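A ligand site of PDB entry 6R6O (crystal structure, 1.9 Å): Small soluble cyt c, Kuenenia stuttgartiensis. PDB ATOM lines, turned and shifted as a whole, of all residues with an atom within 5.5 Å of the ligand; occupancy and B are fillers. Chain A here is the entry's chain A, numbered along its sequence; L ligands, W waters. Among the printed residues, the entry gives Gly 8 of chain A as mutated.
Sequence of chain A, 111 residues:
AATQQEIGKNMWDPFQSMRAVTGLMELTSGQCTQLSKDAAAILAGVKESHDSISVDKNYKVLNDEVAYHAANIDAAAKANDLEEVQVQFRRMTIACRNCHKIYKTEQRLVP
The side-chain sulfur of Cys 96 is bonded to a carbon (C18) of the ligand, at 1.8 Å. SG of Cys 99 is covalently linked to C25 of the ligand, 1.8 Å away. A ring nitrogen (NE2) of His 100 is bound to an iron atom (FE1) of the ligand (2.2 Å). NE2 of Gln 5 is in hydrogen-bond range of O2 of the ligand (3.1 Å). The side-chain amino group of Lys 104 is in salt-bridge range of an oxygen (O3) of the ligand, at 3.3 Å.
ND1 of His 100 sits close to O of Val 110. The side-chain amide nitrogen of Asn 63 sits at hydrogen-bond distance from the side-chain hydroxyl of Ser 49, 2.9 Å away. The side-chain amide oxygen of Gln 4 lies within hydrogen-bond range of the side-chain hydroxyl of Tyr 59. The side-chain amide oxygen (OE1) of Gln 4 is in hydrogen-bond range of the side-chain hydroxyl (OG) of Ser 49 (2.5 Å). The backbone NH of Tyr 59 sits at hydrogen-bond distance from the side-chain hydroxyl of Tyr 103 (3.4 Å).
Merely in contact with the ligand: Gln 4 (3.4 Å), Gly 8 (3.6 Å), Lys 9 (3.1 Å), Met 11 (3.7 Å), Trp 12 (3.96 Å), Phe 15 (3.8 Å), Ile 42 (3.7 Å), Tyr 59 (3.5 Å), Leu 62 (3.9 Å), Asn 63 (3.3 Å), Val 66 (3.6 Å), Leu 109 (3.8 Å) and Val 110 (3.7 Å). Within 4 Å of the ligand: Gln 4, Gln 5, Gly 8, Lys 9, Met 11, Trp 12, Phe 15, Ile 42, Tyr 59, Leu 62, Asn 63, Val 66, Cys 96, Cys 99, His 100, Lys 104, Leu 109 and Val 110. Along chain A the residues within 4 Å of the ligand span positions 4 to 110. The nearest printed residue that does not touch the ligand is Met 92 (4.1 Å).
Water W2 lies within hydrogen-bond range of the side-chain amide nitrogen of Gln 4 and the backbone NH of Gly 8. Water W1 bridges O4 of the ligand and NE2 of Gln 107.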
ATOM      1  N   GLN A   4       9.889 -30.912  27.970  1.00  0.00           N
ATOM      2  CA  GLN A   4      10.456 -29.574  27.897  1.00  0.00           C
ATOM      3  C   GLN A   4       9.506 -28.553  28.512  1.00  0.00           C
ATOM      4  O   GLN A   4       9.948 -27.638  29.217  1.00  0.00           O
ATOM      5  CB  GLN A   4      10.787 -29.205  26.450  1.00  0.00           C
ATOM      6  CG  GLN A   4      11.443 -27.827  26.360  1.00  0.00           C
ATOM      7  CD  GLN A   4      12.838 -27.791  26.965  1.00  0.00           C
ATOM      8  OE1 GLN A   4      13.731 -28.539  26.538  1.00  0.00           O
ATOM      9  NE2 GLN A   4      13.036 -26.927  27.960  1.00  0.00           N
ATOM     10  N   GLN A   5       8.190 -28.729  28.313  1.00  0.00           N
ATOM     11  CA  GLN A   5       7.230 -27.796  28.902  1.00  0.00           C
ATOM     12  C   GLN A   5       7.295 -27.803  30.429  1.00  0.00           C
ATOM     13  O   GLN A   5       7.176 -26.750  31.063  1.00  0.00           O
ATOM     14  CB  GLN A   5       5.823 -28.126  28.437  1.00  0.00           C
ATOM     15  CG  GLN A   5       4.777 -27.133  28.880  1.00  0.00           C
ATOM     16  CD  GLN A   5       3.410 -27.450  28.323  1.00  0.00           C
ATOM     17  OE1 GLN A   5       3.207 -28.497  27.716  1.00  0.00           O
ATOM     18  NE2 GLN A   5       2.462 -26.532  28.519  1.00  0.00           N
ATOM     19  N   GLY A   8      10.349 -25.802  31.470  1.00  0.00           N
ATOM     20  CA  GLY A   8      10.126 -24.362  31.372  1.00  0.00           C
ATOM     21  C   GLY A   8       9.274 -23.837  32.503  1.00  0.00           C
ATOM     22  O   GLY A   8       9.564 -22.787  33.087  1.00  0.00           O
ATOM     23  N   LYS A   9       8.185 -24.553  32.826  1.00  0.00           N
ATOM     24  CA  LYS A   9       7.352 -24.167  33.955  1.00  0.00           C
ATOM     25  C   LYS A   9       8.189 -24.073  35.235  1.00  0.00           C
ATOM     26  O   LYS A   9       8.107 -23.084  35.965  1.00  0.00           O
ATOM     27  CB  LYS A   9       6.210 -25.175  34.142  1.00  0.00           C
ATOM     28  CG  LYS A   9       5.056 -24.969  33.183  1.00  0.00           C
ATOM     29  CD  LYS A   9       3.977 -26.023  33.366  1.00  0.00           C
ATOM     30  CE  LYS A   9       2.807 -25.804  32.419  1.00  0.00           C
ATOM     31  NZ  LYS A   9       1.895 -26.981  32.397  1.00  0.00           N
ATOM     32  N   MET A  11      11.278 -23.507  35.535  1.00  0.00           N
ATOM     33  CA  MET A  11      12.289 -22.466  35.453  1.00  0.00           C
ATOM     34  C   MET A  11      11.707 -21.060  35.565  1.00  0.00           C
ATOM     35  O   MET A  11      12.462 -20.104  35.771  1.00  0.00           O
ATOM     36  CB  MET A  11      13.080 -22.578  34.156  1.00  0.00           C
ATOM     37  CG  MET A  11      14.053 -23.735  34.141  1.00  0.00           C
ATOM     38  SD  MET A  11      15.404 -23.499  32.961  1.00  0.00           S
ATOM     39  CE  MET A  11      14.523 -23.583  31.425  1.00  0.00           C
ATOM     40  N   TRP A  12      10.388 -20.913  35.441  1.00  0.00           N
ATOM     41  CA  TRP A  12       9.783 -19.591  35.379  1.00  0.00           C
ATOM     42  C   TRP A  12       9.929 -18.846  36.717  1.00  0.00           C
ATOM     43  O   TRP A  12      10.294 -17.665  36.734  1.00  0.00           O
ATOM     44  CB  TRP A  12       8.315 -19.708  34.978  1.00  0.00           C
ATOM     45  CG  TRP A  12       7.660 -18.415  34.728  1.00  0.00           C
ATOM     46  CD1 TRP A  12       6.507 -17.955  35.293  1.00  0.00           C
ATOM     47  CD2 TRP A  12       8.125 -17.371  33.851  1.00  0.00           C
ATOM     48  NE1 TRP A  12       6.216 -16.699  34.816  1.00  0.00           N
ATOM     49  CE2 TRP A  12       7.189 -16.322  33.936  1.00  0.00           C
ATOM     50  CE3 TRP A  12       9.228 -17.233  33.007  1.00  0.00           C
ATOM     51  CZ2 TRP A  12       7.332 -15.139  33.199  1.00  0.00           C
ATOM     52  CZ3 TRP A  12       9.367 -16.055  32.286  1.00  0.00           C
ATOM     53  CH2 TRP A  12       8.429 -15.030  32.394  1.00  0.00           C
ATOM     54  N   PHE A  15      13.452 -17.741  37.198  1.00  0.00           N
ATOM     55  CA  PHE A  15      13.780 -16.651  36.271  1.00  0.00           C
ATOM     56  C   PHE A  15      13.117 -15.355  36.708  1.00  0.00           C
ATOM     57  O   PHE A  15      13.744 -14.292  36.658  1.00  0.00           O
ATOM     58  CB  PHE A  15      13.354 -17.039  34.841  1.00  0.00           C
ATOM     59  CG  PHE A  15      13.463 -15.913  33.841  1.00  0.00           C
ATOM     60  CD1 PHE A  15      12.474 -14.929  33.731  1.00  0.00           C
ATOM     61  CD2 PHE A  15      14.605 -15.783  33.044  1.00  0.00           C
ATOM     62  CE1 PHE A  15      12.586 -13.905  32.800  1.00  0.00           C
ATOM     63  CE2 PHE A  15      14.729 -14.746  32.114  1.00  0.00           C
ATOM     64  CZ  PHE A  15      13.719 -13.796  32.005  1.00  0.00           C
ATOM     65  N   ILE A  42      18.164 -22.779  37.226  1.00  0.00           N
ATOM     66  CA  ILE A  42      18.192 -22.675  35.771  1.00  0.00           C
ATOM     67  C   ILE A  42      19.217 -23.619  35.185  1.00  0.00           C
ATOM     68  O   ILE A  42      18.938 -24.349  34.230  1.00  0.00           O
ATOM     69  CB  ILE A  42      18.477 -21.226  35.347  1.00  0.00           C
ATOM     70  CG1 ILE A  42      17.408 -20.279  35.902  1.00  0.00           C
ATOM     71  CG2 ILE A  42      18.684 -21.163  33.831  1.00  0.00           C
ATOM     72  CD1 ILE A  42      16.152 -20.223  35.097  1.00  0.00           C
ATOM     73  N   VAL A  46      18.299 -26.508  32.343  1.00  0.00           N
ATOM     74  CA  VAL A  46      18.813 -26.650  30.990  1.00  0.00           C
ATOM     75  C   VAL A  46      19.708 -27.867  30.882  1.00  0.00           C
ATOM     76  O   VAL A  46      19.844 -28.454  29.807  1.00  0.00           O
ATOM     77  CB  VAL A  46      19.519 -25.353  30.522  1.00  0.00           C
ATOM     78  CG1 VAL A  46      18.532 -24.190  30.528  1.00  0.00           C
ATOM     79  CG2 VAL A  46      20.739 -25.061  31.368  1.00  0.00           C
ATOM     80  N   SER A  49      17.119 -30.674  30.290  1.00  0.00           N
ATOM     81  CA  SER A  49      16.680 -30.611  28.904  1.00  0.00           C
ATOM     82  C   SER A  49      17.783 -31.049  27.952  1.00  0.00           C
ATOM     83  O   SER A  49      17.573 -31.893  27.068  1.00  0.00           O
ATOM     84  CB  SER A  49      16.222 -29.188  28.553  1.00  0.00           C
ATOM     85  OG  SER A  49      16.071 -29.020  27.160  1.00  0.00           O
ATOM     86  N   TYR A  59      19.809 -27.829  19.477  1.00  0.00           N
ATOM     87  CA  TYR A  59      19.092 -27.794  20.746  1.00  0.00           C
ATOM     88  C   TYR A  59      20.059 -27.876  21.917  1.00  0.00           C
ATOM     89  O   TYR A  59      19.917 -27.178  22.920  1.00  0.00           O
ATOM     90  CB  TYR A  59      18.093 -28.962  20.777  1.00  0.00           C
ATOM     91  CG  TYR A  59      16.897 -28.775  21.682  1.00  0.00           C
ATOM     92  CD1 TYR A  59      15.789 -28.064  21.230  1.00  0.00           C
ATOM     93  CD2 TYR A  59      16.858 -29.317  22.970  1.00  0.00           C
ATOM     94  CE1 TYR A  59      14.688 -27.887  22.022  1.00  0.00           C
ATOM     95  CE2 TYR A  59      15.736 -29.132  23.789  1.00  0.00           C
ATOM     96  CZ  TYR A  59      14.654 -28.424  23.294  1.00  0.00           C
ATOM     97  OH  TYR A  59      13.525 -28.225  24.039  1.00  0.00           O
ATOM     98  N   LEU A  62      22.017 -24.527  22.221  1.00  0.00           N
ATOM     99  CA  LEU A  62      21.168 -23.478  22.761  1.00  0.00           C
ATOM    100  C   LEU A  62      21.056 -23.592  24.276  1.00  0.00           C
ATOM    101  O   LEU A  62      21.151 -22.593  24.993  1.00  0.00           O
ATOM    102  CB  LEU A  62      19.773 -23.525  22.127  1.00  0.00           C
ATOM    103  CG  LEU A  62      19.725 -23.000  20.693  1.00  0.00           C
ATOM    104  CD1 LEU A  62      18.599 -23.670  19.928  1.00  0.00           C
ATOM    105  CD2 LEU A  62      19.577 -21.482  20.706  1.00  0.00           C
ATOM    106  N   ASN A  63      20.809 -24.812  24.767  1.00  0.00           N
ATOM    107  CA  ASN A  63      20.817 -25.037  26.206  1.00  0.00           C
ATOM    108  C   ASN A  63      22.135 -24.624  26.830  1.00  0.00           C
ATOM    109  O   ASN A  63      22.161 -23.960  27.878  1.00  0.00           O
ATOM    110  CB  ASN A  63      20.537 -26.516  26.501  1.00  0.00           C
ATOM    111  CG  ASN A  63      19.058 -26.809  26.721  1.00  0.00           C
ATOM    112  OD1 ASN A  63      18.372 -26.087  27.442  1.00  0.00           O
ATOM    113  ND2 ASN A  63      18.574 -27.879  26.104  1.00  0.00           N
ATOM    114  N   VAL A  66      22.355 -20.798  27.309  1.00  0.00           N
ATOM    115  CA  VAL A  66      21.680 -20.390  28.543  1.00  0.00           C
ATOM    116  C   VAL A  66      22.562 -20.701  29.746  1.00  0.00           C
ATOM    117  O   VAL A  66      22.761 -19.848  30.630  1.00  0.00           O
ATOM    118  CB  VAL A  66      20.304 -21.053  28.672  1.00  0.00           C
ATOM    119  CG1 VAL A  66      19.773 -20.854  30.063  1.00  0.00           C
ATOM    120  CG2 VAL A  66      19.333 -20.486  27.652  1.00  0.00           C
ATOM    121  N   MET A  92      21.305 -13.863  29.138  1.00  0.00           N
ATOM    122  CA  MET A  92      20.614 -15.138  29.334  1.00  0.00           C
ATOM    123  C   MET A  92      19.190 -15.066  28.818  1.00  0.00           C
ATOM    124  O   MET A  92      18.667 -16.049  28.269  1.00  0.00           O
ATOM    125  CB  MET A  92      20.617 -15.531  30.816  1.00  0.00           C
ATOM    126  CG  MET A  92      20.061 -16.919  31.059  1.00  0.00           C
ATOM    127  SD  MET A  92      19.812 -17.275  32.807  1.00  0.00           S
ATOM    128  CE  MET A  92      18.287 -16.395  33.146  1.00  0.00           C
ATOM    129  N   ALA A  95      19.256 -15.732  25.327  1.00  0.00           N
ATOM    130  CA  ALA A  95      19.512 -17.150  25.088  1.00  0.00           C
ATOM    131  C   ALA A  95      18.233 -17.992  25.250  1.00  0.00           C
ATOM    132  O   ALA A  95      17.947 -18.867  24.422  1.00  0.00           O
ATOM    133  CB  ALA A  95      20.610 -17.657  26.020  1.00  0.00           C
ATOM    134  N   CYS A  96      17.459 -17.733  26.311  1.00  0.00           N
ATOM    135  CA  CYS A  96      16.145 -18.388  26.436  1.00  0.00           C
ATOM    136  C   CYS A  96      15.303 -18.131  25.195  1.00  0.00           C
ATOM    137  O   CYS A  96      14.743 -19.062  24.601  1.00  0.00           O
ATOM    138  CB  CYS A  96      15.396 -17.871  27.671  1.00  0.00           C
ATOM    139  SG  CYS A  96      16.193 -17.959  29.270  1.00  0.00           S
ATOM    140  N   CYS A  99      16.011 -20.087  21.749  1.00  0.00           N
ATOM    141  CA  CYS A  99      15.458 -21.425  21.548  1.00  0.00           C
ATOM    142  C   CYS A  99      13.960 -21.369  21.289  1.00  0.00           C
ATOM    143  O   CYS A  99      13.458 -22.011  20.366  1.00  0.00           O
ATOM    144  CB  CYS A  99      15.763 -22.329  22.731  1.00  0.00           C
ATOM    145  SG  CYS A  99      15.207 -24.008  22.385  1.00  0.00           S
ATOM    146  N   HIS A 100      13.236 -20.560  22.078  1.00  0.00           N
ATOM    147  CA  HIS A 100      11.795 -20.415  21.885  1.00  0.00           C
ATOM    148  C   HIS A 100      11.453 -19.981  20.466  1.00  0.00           C
ATOM    149  O   HIS A 100      10.519 -20.512  19.842  1.00  0.00           O
ATOM    150  CB  HIS A 100      11.246 -19.389  22.880  1.00  0.00           C
ATOM    151  CG  HIS A 100      11.277 -19.859  24.295  1.00  0.00           C
ATOM    152  ND1 HIS A 100      11.010 -19.014  25.359  1.00  0.00           N
ATOM    153  CD2 HIS A 100      11.529 -21.073  24.837  1.00  0.00           C
ATOM    154  CE1 HIS A 100      11.102 -19.699  26.488  1.00  0.00           C
ATOM    155  NE2 HIS A 100      11.413 -20.946  26.196  1.00  0.00           N
ATOM    156  N   TYR A 103      12.492 -23.033  17.908  1.00  0.00           N
ATOM    157  CA  TYR A 103      11.809 -24.321  18.013  1.00  0.00           C
ATOM    158  C   TYR A 103      10.320 -24.214  18.286  1.00  0.00           C
ATOM    159  O   TYR A 103       9.581 -25.151  17.984  1.00  0.00           O
ATOM    160  CB  TYR A 103      12.490 -25.202  19.089  1.00  0.00           C
ATOM    161  CG  TYR A 103      13.812 -25.778  18.606  1.00  0.00           C
ATOM    162  CD1 TYR A 103      14.985 -25.034  18.645  1.00  0.00           C
ATOM    163  CD2 TYR A 103      13.865 -27.059  17.998  1.00  0.00           C
ATOM    164  CE1 TYR A 103      16.181 -25.540  18.166  1.00  0.00           C
ATOM    165  CE2 TYR A 103      15.057 -27.569  17.510  1.00  0.00           C
ATOM    166  CZ  TYR A 103      16.211 -26.804  17.582  1.00  0.00           C
ATOM    167  OH  TYR A 103      17.404 -27.292  17.096  1.00  0.00           O
ATOM    168  N   LYS A 104       9.836 -23.097  18.831  1.00  0.00           N
ATOM    169  CA  LYS A 104       8.395 -22.881  19.059  1.00  0.00           C
ATOM    170  C   LYS A 104       7.964 -21.560  18.443  1.00  0.00           C
ATOM    171  O   LYS A 104       7.352 -20.701  19.073  1.00  0.00           O
ATOM    172  CB  LYS A 104       8.037 -22.934  20.546  1.00  0.00           C
ATOM    173  CG  LYS A 104       8.229 -24.293  21.154  1.00  0.00           C
ATOM    174  CD  LYS A 104       7.342 -25.365  20.517  1.00  0.00           C
ATOM    175  CE  LYS A 104       5.968 -25.410  21.154  1.00  0.00           C
ATOM    176  NZ  LYS A 104       5.189 -26.644  20.805  1.00  0.00           N
ATOM    177  N   GLN A 107       4.319 -20.002  18.650  1.00  0.00           N
ATOM    178  CA  GLN A 107       3.675 -19.903  19.943  1.00  0.00           C
ATOM    179  C   GLN A 107       4.272 -18.722  20.687  1.00  0.00           C
ATOM    180  O   GLN A 107       5.488 -18.514  20.677  1.00  0.00           O
ATOM    181  CB  GLN A 107       3.868 -21.192  20.752  1.00  0.00           C
ATOM    182  CG  GLN A 107       3.457 -21.081  22.207  1.00  0.00           C
ATOM    183  CD  GLN A 107       3.685 -22.373  22.969  1.00  0.00           C
ATOM    184  OE1 GLN A 107       4.046 -23.394  22.380  1.00  0.00           O
ATOM    185  NE2 GLN A 107       3.487 -22.330  24.282  1.00  0.00           N
ATOM    186  N   LEU A 109       5.700 -17.154  23.709  1.00  0.00           N
ATOM    187  CA  LEU A 109       6.322 -17.690  24.906  1.00  0.00           C
ATOM    188  C   LEU A 109       6.990 -16.556  25.668  1.00  0.00           C
ATOM    189  O   LEU A 109       7.335 -15.526  25.099  1.00  0.00           O
ATOM    190  CB  LEU A 109       7.351 -18.777  24.559  1.00  0.00           C
ATOM    191  CG  LEU A 109       6.747 -20.143  24.251  1.00  0.00           C
ATOM    192  CD1 LEU A 109       7.797 -21.100  23.731  1.00  0.00           C
ATOM    193  CD2 LEU A 109       6.089 -20.690  25.485  1.00  0.00           C
ATOM    194  N   VAL A 110       7.118 -16.763  26.971  1.00  0.00           N
ATOM    195  CA  VAL A 110       7.895 -15.869  27.826  1.00  0.00           C
ATOM    196  C   VAL A 110       9.291 -16.479  27.935  1.00  0.00           C
ATOM    197  O   VAL A 110       9.427 -17.698  27.802  1.00  0.00           O
ATOM    198  CB  VAL A 110       7.227 -15.689  29.196  1.00  0.00           C
ATOM    199  CG1 VAL A 110       5.912 -14.954  29.045  1.00  0.00           C
ATOM    200  CG2 VAL A 110       7.000 -17.045  29.857  1.00  0.00           C
ATOM    201  N   PRO A 111      10.342 -15.699  28.190  1.00  0.00           N
ATOM    202  CA  PRO A 111      10.359 -14.257  28.442  1.00  0.00           C
ATOM    203  C   PRO A 111      10.564 -13.446  27.166  1.00  0.00           C
ATOM    204  O   PRO A 111      10.534 -12.214  27.183  1.00  0.00           O
ATOM    205  CB  PRO A 111      11.540 -14.095  29.386  1.00  0.00           C
ATOM    206  CG  PRO A 111      12.515 -15.128  28.895  1.00  0.00           C
ATOM    207  CD  PRO A 111      11.691 -16.287  28.343  1.00  0.00           C
HETATM  208 FE1  LIG L   1      11.850 -22.723  27.485  1.00  0.00          FE
HETATM  209  C1  LIG L   1       8.589 -23.534  27.072  1.00  0.00           C
HETATM  210  C2  LIG L   1      11.038 -20.685  30.118  1.00  0.00           C
HETATM  211  C3  LIG L   1      15.158 -21.741  27.767  1.00  0.00           C
HETATM  212  C4  LIG L   1      12.777 -24.781  24.817  1.00  0.00           C
HETATM  213  N1  LIG L   1      10.148 -22.212  28.434  1.00  0.00           N
HETATM  214  C5  LIG L   1       8.884 -22.655  28.093  1.00  0.00           C
HETATM  215  C6  LIG L   1       7.922 -22.043  28.993  1.00  0.00           C
HETATM  216  C7  LIG L   1       8.595 -21.249  29.828  1.00  0.00           C
HETATM  217  C8  LIG L   1      10.009 -21.347  29.498  1.00  0.00           C
HETATM  218  C9  LIG L   1       7.994 -20.399  30.971  1.00  0.00           C
HETATM  219  C10 LIG L   1       6.390 -22.272  28.959  1.00  0.00           C
HETATM  220  C11 LIG L   1       5.937 -23.289  30.005  1.00  0.00           C
HETATM  221  C12 LIG L   1       4.425 -23.429  29.969  1.00  0.00           C
HETATM  222  O1  LIG L   1       3.769 -23.154  31.001  1.00  0.00           O
HETATM  223  O2  LIG L   1       3.879 -23.810  28.897  1.00  0.00           O
HETATM  224  N2  LIG L   1      12.900 -21.463  28.719  1.00  0.00           N
HETATM  225  C13 LIG L   1      12.354 -20.692  29.726  1.00  0.00           C
HETATM  226  C14 LIG L   1      13.422 -19.898  30.306  1.00  0.00           C
HETATM  227  C15 LIG L   1      14.564 -20.188  29.655  1.00  0.00           C
HETATM  228  C16 LIG L   1      14.250 -21.187  28.638  1.00  0.00           C
HETATM  229  C17 LIG L   1      13.178 -18.883  31.458  1.00  0.00           C
HETATM  230  C18 LIG L   1      15.989 -19.615  29.852  1.00  0.00           C
HETATM  231  C19 LIG L   1      16.432 -19.616  31.336  1.00  0.00           C
HETATM  232  N3  LIG L   1      13.639 -23.189  26.483  1.00  0.00           N
HETATM  233  C20 LIG L   1      14.883 -22.662  26.769  1.00  0.00           C
HETATM  234  C21 LIG L   1      15.847 -23.345  25.935  1.00  0.00           C
HETATM  235  C22 LIG L   1      15.185 -24.096  25.041  1.00  0.00           C
HETATM  236  C23 LIG L   1      13.788 -24.063  25.418  1.00  0.00           C
HETATM  237  C24 LIG L   1      17.319 -22.885  25.863  1.00  0.00           C
HETATM  238  C25 LIG L   1      15.706 -24.931  23.829  1.00  0.00           C
HETATM  239  C26 LIG L   1      16.979 -25.756  24.096  1.00  0.00           C
HETATM  240  N4  LIG L   1      10.865 -23.986  26.169  1.00  0.00           N
HETATM  241  C27 LIG L   1      11.431 -24.669  25.102  1.00  0.00           C
HETATM  242  C28 LIG L   1      10.372 -25.272  24.315  1.00  0.00           C
HETATM  243  C29 LIG L   1       9.079 -24.874  25.021  1.00  0.00           C
HETATM  244  C30 LIG L   1       9.472 -24.085  26.162  1.00  0.00           C
HETATM  245  C31 LIG L   1      10.502 -26.129  23.030  1.00  0.00           C
HETATM  246  C32 LIG L   1       7.651 -25.238  24.613  1.00  0.00           C
HETATM  247  C33 LIG L   1       7.190 -26.385  25.501  1.00  0.00           C
HETATM  248  C34 LIG L   1       5.920 -26.894  24.890  1.00  0.00           C
HETATM  249  O3  LIG L   1       6.025 -27.613  23.876  1.00  0.00           O
HETATM  250  O4  LIG L   1       4.814 -26.554  25.411  1.00  0.00           O
HETATM  251  O   HOH W   1       4.495 -24.256  26.318  1.00  0.00           O
HETATM  252  O   HOH W   2      12.143 -24.383  28.903  1.00  0.00           O
